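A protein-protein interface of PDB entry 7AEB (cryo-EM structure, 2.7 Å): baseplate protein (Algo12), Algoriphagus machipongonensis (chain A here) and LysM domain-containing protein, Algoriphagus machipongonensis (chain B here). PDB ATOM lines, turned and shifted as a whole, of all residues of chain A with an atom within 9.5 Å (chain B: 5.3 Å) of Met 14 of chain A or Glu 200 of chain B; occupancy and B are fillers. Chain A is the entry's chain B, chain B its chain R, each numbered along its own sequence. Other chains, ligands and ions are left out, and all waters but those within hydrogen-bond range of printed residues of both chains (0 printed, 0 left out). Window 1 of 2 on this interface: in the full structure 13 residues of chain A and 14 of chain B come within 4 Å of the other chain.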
ATOM      1  N   ILE A   8     -31.002  41.111  13.494  1.00  0.00           N
ATOM      2  CA  ILE A   8     -30.268  39.889  13.160  1.00  0.00           C
ATOM      3  C   ILE A   8     -28.760  40.096  13.115  1.00  0.00           C
ATOM      4  O   ILE A   8     -28.270  41.009  12.453  1.00  0.00           O
ATOM      5  CB  ILE A   8     -30.749  39.325  11.820  1.00  0.00           C
ATOM      6  CG1 ILE A   8     -32.221  38.938  11.968  1.00  0.00           C
ATOM      7  CG2 ILE A   8     -29.883  38.135  11.385  1.00  0.00           C
ATOM      8  CD1 ILE A   8     -32.914  38.589  10.685  1.00  0.00           C
ATOM      9  N   SER A   9     -28.029  39.209  13.784  1.00  0.00           N
ATOM     10  CA  SER A   9     -26.578  39.246  13.809  1.00  0.00           C
ATOM     11  C   SER A   9     -25.982  37.846  13.799  1.00  0.00           C
ATOM     12  O   SER A   9     -26.688  36.847  13.948  1.00  0.00           O
ATOM     13  CB  SER A   9     -26.083  39.986  15.027  1.00  0.00           C
ATOM     14  OG  SER A   9     -26.451  39.316  16.195  1.00  0.00           O
ATOM     15  N   ILE A  10     -24.664  37.784  13.629  1.00  0.00           N
ATOM     16  CA  ILE A  10     -23.926  36.529  13.572  1.00  0.00           C
ATOM     17  C   ILE A  10     -22.876  36.440  14.678  1.00  0.00           C
ATOM     18  O   ILE A  10     -22.106  37.382  14.886  1.00  0.00           O
ATOM     19  CB  ILE A  10     -23.261  36.307  12.202  1.00  0.00           C
ATOM     20  CG1 ILE A  10     -22.228  37.397  11.921  1.00  0.00           C
ATOM     21  CG2 ILE A  10     -24.308  36.274  11.102  1.00  0.00           C
ATOM     22  CD1 ILE A  10     -21.521  37.256  10.609  1.00  0.00           C
ATOM     23  N   PRO A  11     -22.836  35.304  15.382  1.00  0.00           N
ATOM     24  CA  PRO A  11     -21.901  35.026  16.471  1.00  0.00           C
ATOM     25  C   PRO A  11     -20.472  35.139  16.004  1.00  0.00           C
ATOM     26  O   PRO A  11     -20.193  34.923  14.832  1.00  0.00           O
ATOM     27  CB  PRO A  11     -22.224  33.576  16.825  1.00  0.00           C
ATOM     28  CG  PRO A  11     -23.606  33.367  16.360  1.00  0.00           C
ATOM     29  CD  PRO A  11     -23.767  34.201  15.147  1.00  0.00           C
ATOM     30  N   LYS A  12     -19.573  35.511  16.921  1.00  0.00           N
ATOM     31  CA  LYS A  12     -18.151  35.666  16.600  1.00  0.00           C
ATOM     32  C   LYS A  12     -17.226  34.542  17.102  1.00  0.00           C
ATOM     33  O   LYS A  12     -16.041  34.498  16.741  1.00  0.00           O
ATOM     34  CB  LYS A  12     -17.645  37.020  17.117  1.00  0.00           C
ATOM     35  CG  LYS A  12     -16.189  37.330  16.787  1.00  0.00           C
ATOM     36  CD  LYS A  12     -15.752  38.661  17.289  1.00  0.00           C
ATOM     37  CE  LYS A  12     -14.302  38.942  16.931  1.00  0.00           C
ATOM     38  NZ  LYS A  12     -14.075  38.915  15.461  1.00  0.00           N
ATOM     39  N   ASP A  13     -17.727  33.608  17.899  1.00  0.00           N
ATOM     40  CA  ASP A  13     -16.895  32.512  18.395  1.00  0.00           C
ATOM     41  C   ASP A  13     -17.049  31.267  17.525  1.00  0.00           C
ATOM     42  O   ASP A  13     -17.713  30.294  17.885  1.00  0.00           O
ATOM     43  CB  ASP A  13     -17.243  32.188  19.839  1.00  0.00           C
ATOM     44  CG  ASP A  13     -16.224  31.269  20.499  1.00  0.00           C
ATOM     45  OD1 ASP A  13     -15.136  31.109  19.958  1.00  0.00           O
ATOM     46  OD2 ASP A  13     -16.508  30.745  21.568  1.00  0.00           O
ATOM     47  N   MET A  14     -16.417  31.298  16.363  1.00  0.00           N
ATOM     48  CA  MET A  14     -16.516  30.199  15.406  1.00  0.00           C
ATOM     49  C   MET A  14     -15.598  29.048  15.770  1.00  0.00           C
ATOM     50  O   MET A  14     -14.590  28.811  15.109  1.00  0.00           O
ATOM     51  CB  MET A  14     -16.178  30.680  14.007  1.00  0.00           C
ATOM     52  CG  MET A  14     -17.142  31.670  13.434  1.00  0.00           C
ATOM     53  SD  MET A  14     -18.774  30.980  13.199  1.00  0.00           S
ATOM     54  CE  MET A  14     -19.669  31.623  14.602  1.00  0.00           C
ATOM     55  N   SER A  15     -15.983  28.319  16.810  1.00  0.00           N
ATOM     56  CA  SER A  15     -15.207  27.185  17.304  1.00  0.00           C
ATOM     57  C   SER A  15     -16.123  26.151  17.932  1.00  0.00           C
ATOM     58  O   SER A  15     -16.864  26.458  18.868  1.00  0.00           O
ATOM     59  CB  SER A  15     -14.204  27.657  18.325  1.00  0.00           C
ATOM     60  OG  SER A  15     -13.488  26.578  18.862  1.00  0.00           O
ATOM     61  N   SER A  16     -16.105  24.933  17.421  1.00  0.00           N
ATOM     62  CA  SER A  16     -16.978  23.904  17.975  1.00  0.00           C
ATOM     63  C   SER A  16     -16.284  22.586  18.198  1.00  0.00           C
ATOM     64  O   SER A  16     -16.785  21.759  18.971  1.00  0.00           O
ATOM     65  CB  SER A  16     -18.160  23.676  17.060  1.00  0.00           C
ATOM     66  OG  SER A  16     -17.697  23.216  15.828  1.00  0.00           O
ATOM     67  N   LYS A  17     -15.142  22.376  17.561  1.00  0.00           N
ATOM     68  CA  LYS A  17     -14.417  21.115  17.643  1.00  0.00           C
ATOM     69  C   LYS A  17     -15.249  19.920  17.177  1.00  0.00           C
ATOM     70  O   LYS A  17     -15.205  18.847  17.780  1.00  0.00           O
ATOM     71  CB  LYS A  17     -13.914  20.855  19.064  1.00  0.00           C
ATOM     72  CG  LYS A  17     -13.188  22.016  19.729  1.00  0.00           C
ATOM     73  CD  LYS A  17     -11.912  22.384  18.999  1.00  0.00           C
ATOM     74  CE  LYS A  17     -11.150  23.467  19.741  1.00  0.00           C
ATOM     75  NZ  LYS A  17      -9.993  23.975  18.951  1.00  0.00           N
ATOM     76  N   ASP A  18     -15.998  20.098  16.092  1.00  0.00           N
ATOM     77  CA  ASP A  18     -16.823  19.044  15.514  1.00  0.00           C
ATOM     78  C   ASP A  18     -16.787  19.129  13.988  1.00  0.00           C
ATOM     79  O   ASP A  18     -15.930  19.791  13.408  1.00  0.00           O
ATOM     80  CB  ASP A  18     -18.241  19.094  16.094  1.00  0.00           C
ATOM     81  CG  ASP A  18     -18.975  20.376  15.805  1.00  0.00           C
ATOM     82  OD1 ASP A  18     -18.712  21.023  14.798  1.00  0.00           O
ATOM     83  OD2 ASP A  18     -19.832  20.743  16.592  1.00  0.00           O
ATOM     84  N   LEU A  20     -18.486  20.727  11.859  1.00  0.00           N
ATOM     85  CA  LEU A  20     -18.779  21.992  11.218  1.00  0.00           C
ATOM     86  C   LEU A  20     -17.618  22.975  11.341  1.00  0.00           C
ATOM     87  O   LEU A  20     -17.698  24.108  10.858  1.00  0.00           O
ATOM     88  CB  LEU A  20     -20.039  22.580  11.835  1.00  0.00           C
ATOM     89  CG  LEU A  20     -21.294  21.708  11.748  1.00  0.00           C
ATOM     90  CD1 LEU A  20     -22.401  22.390  12.461  1.00  0.00           C
ATOM     91  CD2 LEU A  20     -21.684  21.439  10.305  1.00  0.00           C
ATOM     92  N   ASP A  21     -16.546  22.560  11.996  1.00  0.00           N
ATOM     93  CA  ASP A  21     -15.377  23.394  12.258  1.00  0.00           C
ATOM     94  C   ASP A  21     -14.234  23.039  11.298  1.00  0.00           C
ATOM     95  O   ASP A  21     -13.530  22.047  11.493  1.00  0.00           O
ATOM     96  CB  ASP A  21     -15.038  23.205  13.739  1.00  0.00           C
ATOM     97  CG  ASP A  21     -13.889  24.000  14.276  1.00  0.00           C
ATOM     98  OD1 ASP A  21     -12.993  24.387  13.523  1.00  0.00           O
ATOM     99  OD2 ASP A  21     -13.883  24.210  15.514  1.00  0.00           O
ATOM    100  N   PHE A  22     -14.050  23.865  10.267  1.00  0.00           N
ATOM    101  CA  PHE A  22     -13.058  23.584   9.227  1.00  0.00           C
ATOM    102  C   PHE A  22     -11.656  23.419   9.778  1.00  0.00           C
ATOM    103  O   PHE A  22     -10.943  22.488   9.400  1.00  0.00           O
ATOM    104  CB  PHE A  22     -13.023  24.689   8.187  1.00  0.00           C
ATOM    105  CG  PHE A  22     -11.985  24.464   7.134  1.00  0.00           C
ATOM    106  CD1 PHE A  22     -12.244  23.655   6.051  1.00  0.00           C
ATOM    107  CD2 PHE A  22     -10.737  25.048   7.230  1.00  0.00           C
ATOM    108  CE1 PHE A  22     -11.281  23.443   5.093  1.00  0.00           C
ATOM    109  CE2 PHE A  22      -9.787  24.824   6.290  1.00  0.00           C
ATOM    110  CZ  PHE A  22     -10.057  24.025   5.216  1.00  0.00           C
ATOM    111  N   HIS A  23     -11.227  24.344  10.620  1.00  0.00           N
ATOM    112  CA  HIS A  23      -9.856  24.304  11.087  1.00  0.00           C
ATOM    113  C   HIS A  23      -9.611  23.091  11.945  1.00  0.00           C
ATOM    114  O   HIS A  23      -8.557  22.462  11.836  1.00  0.00           O
ATOM    115  CB  HIS A  23      -9.534  25.582  11.819  1.00  0.00           C
ATOM    116  CG  HIS A  23      -9.458  26.731  10.886  1.00  0.00           C
ATOM    117  ND1 HIS A  23      -8.457  26.857   9.954  1.00  0.00           N
ATOM    118  CD2 HIS A  23     -10.284  27.776  10.698  1.00  0.00           C
ATOM    119  CE1 HIS A  23      -8.661  27.945   9.240  1.00  0.00           C
ATOM    120  NE2 HIS A  23      -9.761  28.522   9.675  1.00  0.00           N
ATOM    121  N   PHE A  24     -10.586  22.730  12.762  1.00  0.00           N
ATOM    122  CA  PHE A  24     -10.473  21.523  13.553  1.00  0.00           C
ATOM    123  C   PHE A  24     -10.269  20.305  12.674  1.00  0.00           C
ATOM    124  O   PHE A  24      -9.365  19.502  12.916  1.00  0.00           O
ATOM    125  CB  PHE A  24     -11.711  21.363  14.389  1.00  0.00           C
ATOM    126  CG  PHE A  24     -11.795  20.121  15.095  1.00  0.00           C
ATOM    127  CD1 PHE A  24     -11.046  19.903  16.209  1.00  0.00           C
ATOM    128  CD2 PHE A  24     -12.664  19.163  14.670  1.00  0.00           C
ATOM    129  CE1 PHE A  24     -11.158  18.735  16.881  1.00  0.00           C
ATOM    130  CE2 PHE A  24     -12.778  17.997  15.332  1.00  0.00           C
ATOM    131  CZ  PHE A  24     -12.026  17.781  16.444  1.00  0.00           C
ATOM    132  N   ASN A  66     -23.904  20.420   7.740  1.00  0.00           N
ATOM    133  CA  ASN A  66     -24.868  21.497   7.728  1.00  0.00           C
ATOM    134  C   ASN A  66     -26.250  21.052   7.276  1.00  0.00           C
ATOM    135  O   ASN A  66     -27.245  21.589   7.765  1.00  0.00           O
ATOM    136  CB  ASN A  66     -24.359  22.610   6.848  1.00  0.00           C
ATOM    137  CG  ASN A  66     -25.163  23.827   6.964  1.00  0.00           C
ATOM    138  OD1 ASN A  66     -25.261  24.421   8.033  1.00  0.00           O
ATOM    139  ND2 ASN A  66     -25.753  24.229   5.873  1.00  0.00           N
ATOM    140  N   LYS B 196     -13.686  32.342   7.672  1.00  0.00           N
ATOM    141  CA  LYS B 196     -14.257  31.306   8.519  1.00  0.00           C
ATOM    142  C   LYS B 196     -15.731  31.519   8.833  1.00  0.00           C
ATOM    143  O   LYS B 196     -16.348  30.643   9.443  1.00  0.00           O
ATOM    144  CB  LYS B 196     -13.465  31.215   9.816  1.00  0.00           C
ATOM    145  CG  LYS B 196     -13.550  32.470  10.643  1.00  0.00           C
ATOM    146  CD  LYS B 196     -12.771  32.349  11.924  1.00  0.00           C
ATOM    147  CE  LYS B 196     -13.021  33.552  12.802  1.00  0.00           C
ATOM    148  NZ  LYS B 196     -12.442  33.383  14.154  1.00  0.00           N
ATOM    149  N   TYR B 197     -16.314  32.643   8.434  1.00  0.00           N
ATOM    150  CA  TYR B 197     -17.707  32.940   8.751  1.00  0.00           C
ATOM    151  C   TYR B 197     -18.687  32.483   7.682  1.00  0.00           C
ATOM    152  O   TYR B 197     -19.848  32.892   7.736  1.00  0.00           O
ATOM    153  CB  TYR B 197     -17.898  34.441   8.971  1.00  0.00           C
ATOM    154  CG  TYR B 197     -17.160  35.001  10.153  1.00  0.00           C
ATOM    155  CD1 TYR B 197     -17.550  34.695  11.445  1.00  0.00           C
ATOM    156  CD2 TYR B 197     -16.081  35.851   9.978  1.00  0.00           C
ATOM    157  CE1 TYR B 197     -16.882  35.208  12.527  1.00  0.00           C
ATOM    158  CE2 TYR B 197     -15.405  36.365  11.052  1.00  0.00           C
ATOM    159  CZ  TYR B 197     -15.813  36.042  12.323  1.00  0.00           C
ATOM    160  OH  TYR B 197     -15.147  36.558  13.404  1.00  0.00           O
ATOM    161  N   TYR B 198     -18.257  31.642   6.733  1.00  0.00           N
ATOM    162  CA  TYR B 198     -19.089  31.298   5.582  1.00  0.00           C
ATOM    163  C   TYR B 198     -20.305  30.453   5.956  1.00  0.00           C
ATOM    164  O   TYR B 198     -21.318  30.492   5.254  1.00  0.00           O
ATOM    165  CB  TYR B 198     -18.249  30.580   4.512  1.00  0.00           C
ATOM    166  CG  TYR B 198     -17.763  29.197   4.898  1.00  0.00           C
ATOM    167  CD1 TYR B 198     -16.617  29.033   5.660  1.00  0.00           C
ATOM    168  CD2 TYR B 198     -18.442  28.055   4.486  1.00  0.00           C
ATOM    169  CE1 TYR B 198     -16.174  27.783   6.021  1.00  0.00           C
ATOM    170  CE2 TYR B 198     -18.009  26.803   4.848  1.00  0.00           C
ATOM    171  CZ  TYR B 198     -16.872  26.673   5.611  1.00  0.00           C
ATOM    172  OH  TYR B 198     -16.425  25.431   5.972  1.00  0.00           O
ATOM    173  N   LEU B 199     -20.232  29.678   7.039  1.00  0.00           N
ATOM    174  CA  LEU B 199     -21.399  28.899   7.436  1.00  0.00           C
ATOM    175  C   LEU B 199     -22.434  29.733   8.176  1.00  0.00           C
ATOM    176  O   LEU B 199     -23.591  29.317   8.270  1.00  0.00           O
ATOM    177  CB  LEU B 199     -20.997  27.704   8.300  1.00  0.00           C
ATOM    178  CG  LEU B 199     -20.594  26.412   7.586  1.00  0.00           C
ATOM    179  CD1 LEU B 199     -20.354  25.299   8.581  1.00  0.00           C
ATOM    180  CD2 LEU B 199     -21.640  26.001   6.582  1.00  0.00           C
ATOM    181  N   GLU B 200     -22.056  30.892   8.705  1.00  0.00           N
ATOM    182  CA  GLU B 200     -23.043  31.766   9.324  1.00  0.00           C
ATOM    183  C   GLU B 200     -23.730  32.642   8.287  1.00  0.00           C
ATOM    184  O   GLU B 200     -24.880  33.047   8.478  1.00  0.00           O
ATOM    185  CB  GLU B 200     -22.384  32.623  10.401  1.00  0.00           C
ATOM    186  CG  GLU B 200     -21.812  31.839  11.552  1.00  0.00           C
ATOM    187  CD  GLU B 200     -22.868  31.079  12.322  1.00  0.00           C
ATOM    188  OE1 GLU B 200     -23.969  31.626  12.537  1.00  0.00           O
ATOM    189  OE2 GLU B 200     -22.597  29.927  12.720  1.00  0.00           O
ATOM    190  N   VAL B 201     -23.036  32.950   7.192  1.00  0.00           N
ATOM    191  CA  VAL B 201     -23.646  33.705   6.105  1.00  0.00           C
ATOM    192  C   VAL B 201     -24.644  32.832   5.357  1.00  0.00           C
ATOM    193  O   VAL B 201     -25.695  33.307   4.907  1.00  0.00           O
ATOM    194  CB  VAL B 201     -22.548  34.260   5.173  1.00  0.00           C
ATOM    195  CG1 VAL B 201     -23.133  35.064   4.023  1.00  0.00           C
ATOM    196  CG2 VAL B 201     -21.582  35.112   5.954  1.00  0.00           C
ATOM    197  N   ALA B 202     -24.353  31.537   5.245  1.00  0.00           N
ATOM    198  CA  ALA B 202     -25.239  30.638   4.518  1.00  0.00           C
ATOM    199  C   ALA B 202     -26.494  30.323   5.321  1.00  0.00           C
ATOM    200  O   ALA B 202     -27.565  30.113   4.746  1.00  0.00           O
ATOM    201  CB  ALA B 202     -24.496  29.354   4.149  1.00  0.00           C
ATOM    202  N   LYS B 203     -26.384  30.296   6.649  1.00  0.00           N
ATOM    203  CA  LYS B 203     -27.547  30.040   7.487  1.00  0.00           C
ATOM    204  C   LYS B 203     -28.468  31.249   7.562  1.00  0.00           C
ATOM    205  O   LYS B 203     -29.684  31.098   7.720  1.00  0.00           O
ATOM    206  CB  LYS B 203     -27.101  29.642   8.889  1.00  0.00           C
ATOM    207  CG  LYS B 203     -27.066  28.163   9.133  1.00  0.00           C
ATOM    208  CD  LYS B 203     -26.746  27.875  10.580  1.00  0.00           C
ATOM    209  CE  LYS B 203     -25.303  28.187  10.888  1.00  0.00           C
ATOM    210  NZ  LYS B 203     -24.945  27.846  12.286  1.00  0.00           N
ATOM    211  N   ALA B 204     -27.913  32.456   7.455  1.00  0.00           N
ATOM    212  CA  ALA B 204     -28.736  33.655   7.526  1.00  0.00           C
ATOM    213  C   ALA B 204     -29.467  33.924   6.222  1.00  0.00           C
ATOM    214  O   ALA B 204     -30.365  34.766   6.185  1.00  0.00           O
ATOM    215  CB  ALA B 204     -27.874  34.857   7.910  1.00  0.00           C
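Glu 200 of chain B touches Pro 11 of chain A.
Met 14 of chain A touches Tyr 197 of chain B (CG to CD1, 3.6 Å).
SD of Met 14 of chain A touches CG of Glu 200 of chain B, at 3.6 Å.
Leu 199 of chain B touches Leu 20 of chain A (CD1 to O, 3.7 Å).
NZ of Lys 12 of chain A sits at hydrogen-bond distance from OH of Tyr 197 of chain B, at 3.3 Å.
Met 14 of chain A touches just these residues of chain B: Tyr 197 and Glu 200.
Glu 200 of chain B touches just these residues of chain A: Pro 11 and Met 14.
No residue of chain A comes within 4 Å of Val 201 of chain B.
No residue of chain A comes within 4 Å of Lys 203 of chain B.
Of the printed residues of chain A, Leu 199 of chain B touches Leu 20.
Of the printed residues of chain A, Tyr 197 of chain B touches Lys 12 and Met 14.
Of the printed residues of chain B, Leu 20 of chain A touches Leu 199 (3.7 Å).
Of the printed residues of chain B, Pro 11 of chain A touches Glu 200.
Ala 202 of chain B touches none of the printed residues of chain A.
Phe 22 of chain A touches none of the printed residues of chain B.
The nearest printed residue of chain A that does not touch Tyr 197 of chain B is Pro 11 of chain A (4.04 Å).
The side-chain carboxylate (OD1) of Asp 18 of chain A lies within hydrogen-bond range of the backbone NH (N) of Leu 20 of chain A, at 3.0 Å.
The side-chain carboxylate (OE2) of Glu 200 of chain B is in salt-bridge range of the side-chain amino group (NZ) of Lys 203 of chain B, at 3.2 Å.
Hydrophobic or aromatic side chains of chain A within 4 Å of the printed part of chain B: Pro 11 and Met 14.
Of the 9 printed residues of chain B, 3 touch a printed residue of chain A.
Hydrophobic or aromatic side chains of chain B within 4 Å of the printed part of chain A: Tyr 197 and Leu 199.
Among the printed residues, 5 pairs touch across the chains.
Among the printed residues, no Asp or Glu carboxylate lies within 4 Å of a Lys or Arg side-chain nitrogen of the other chain.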
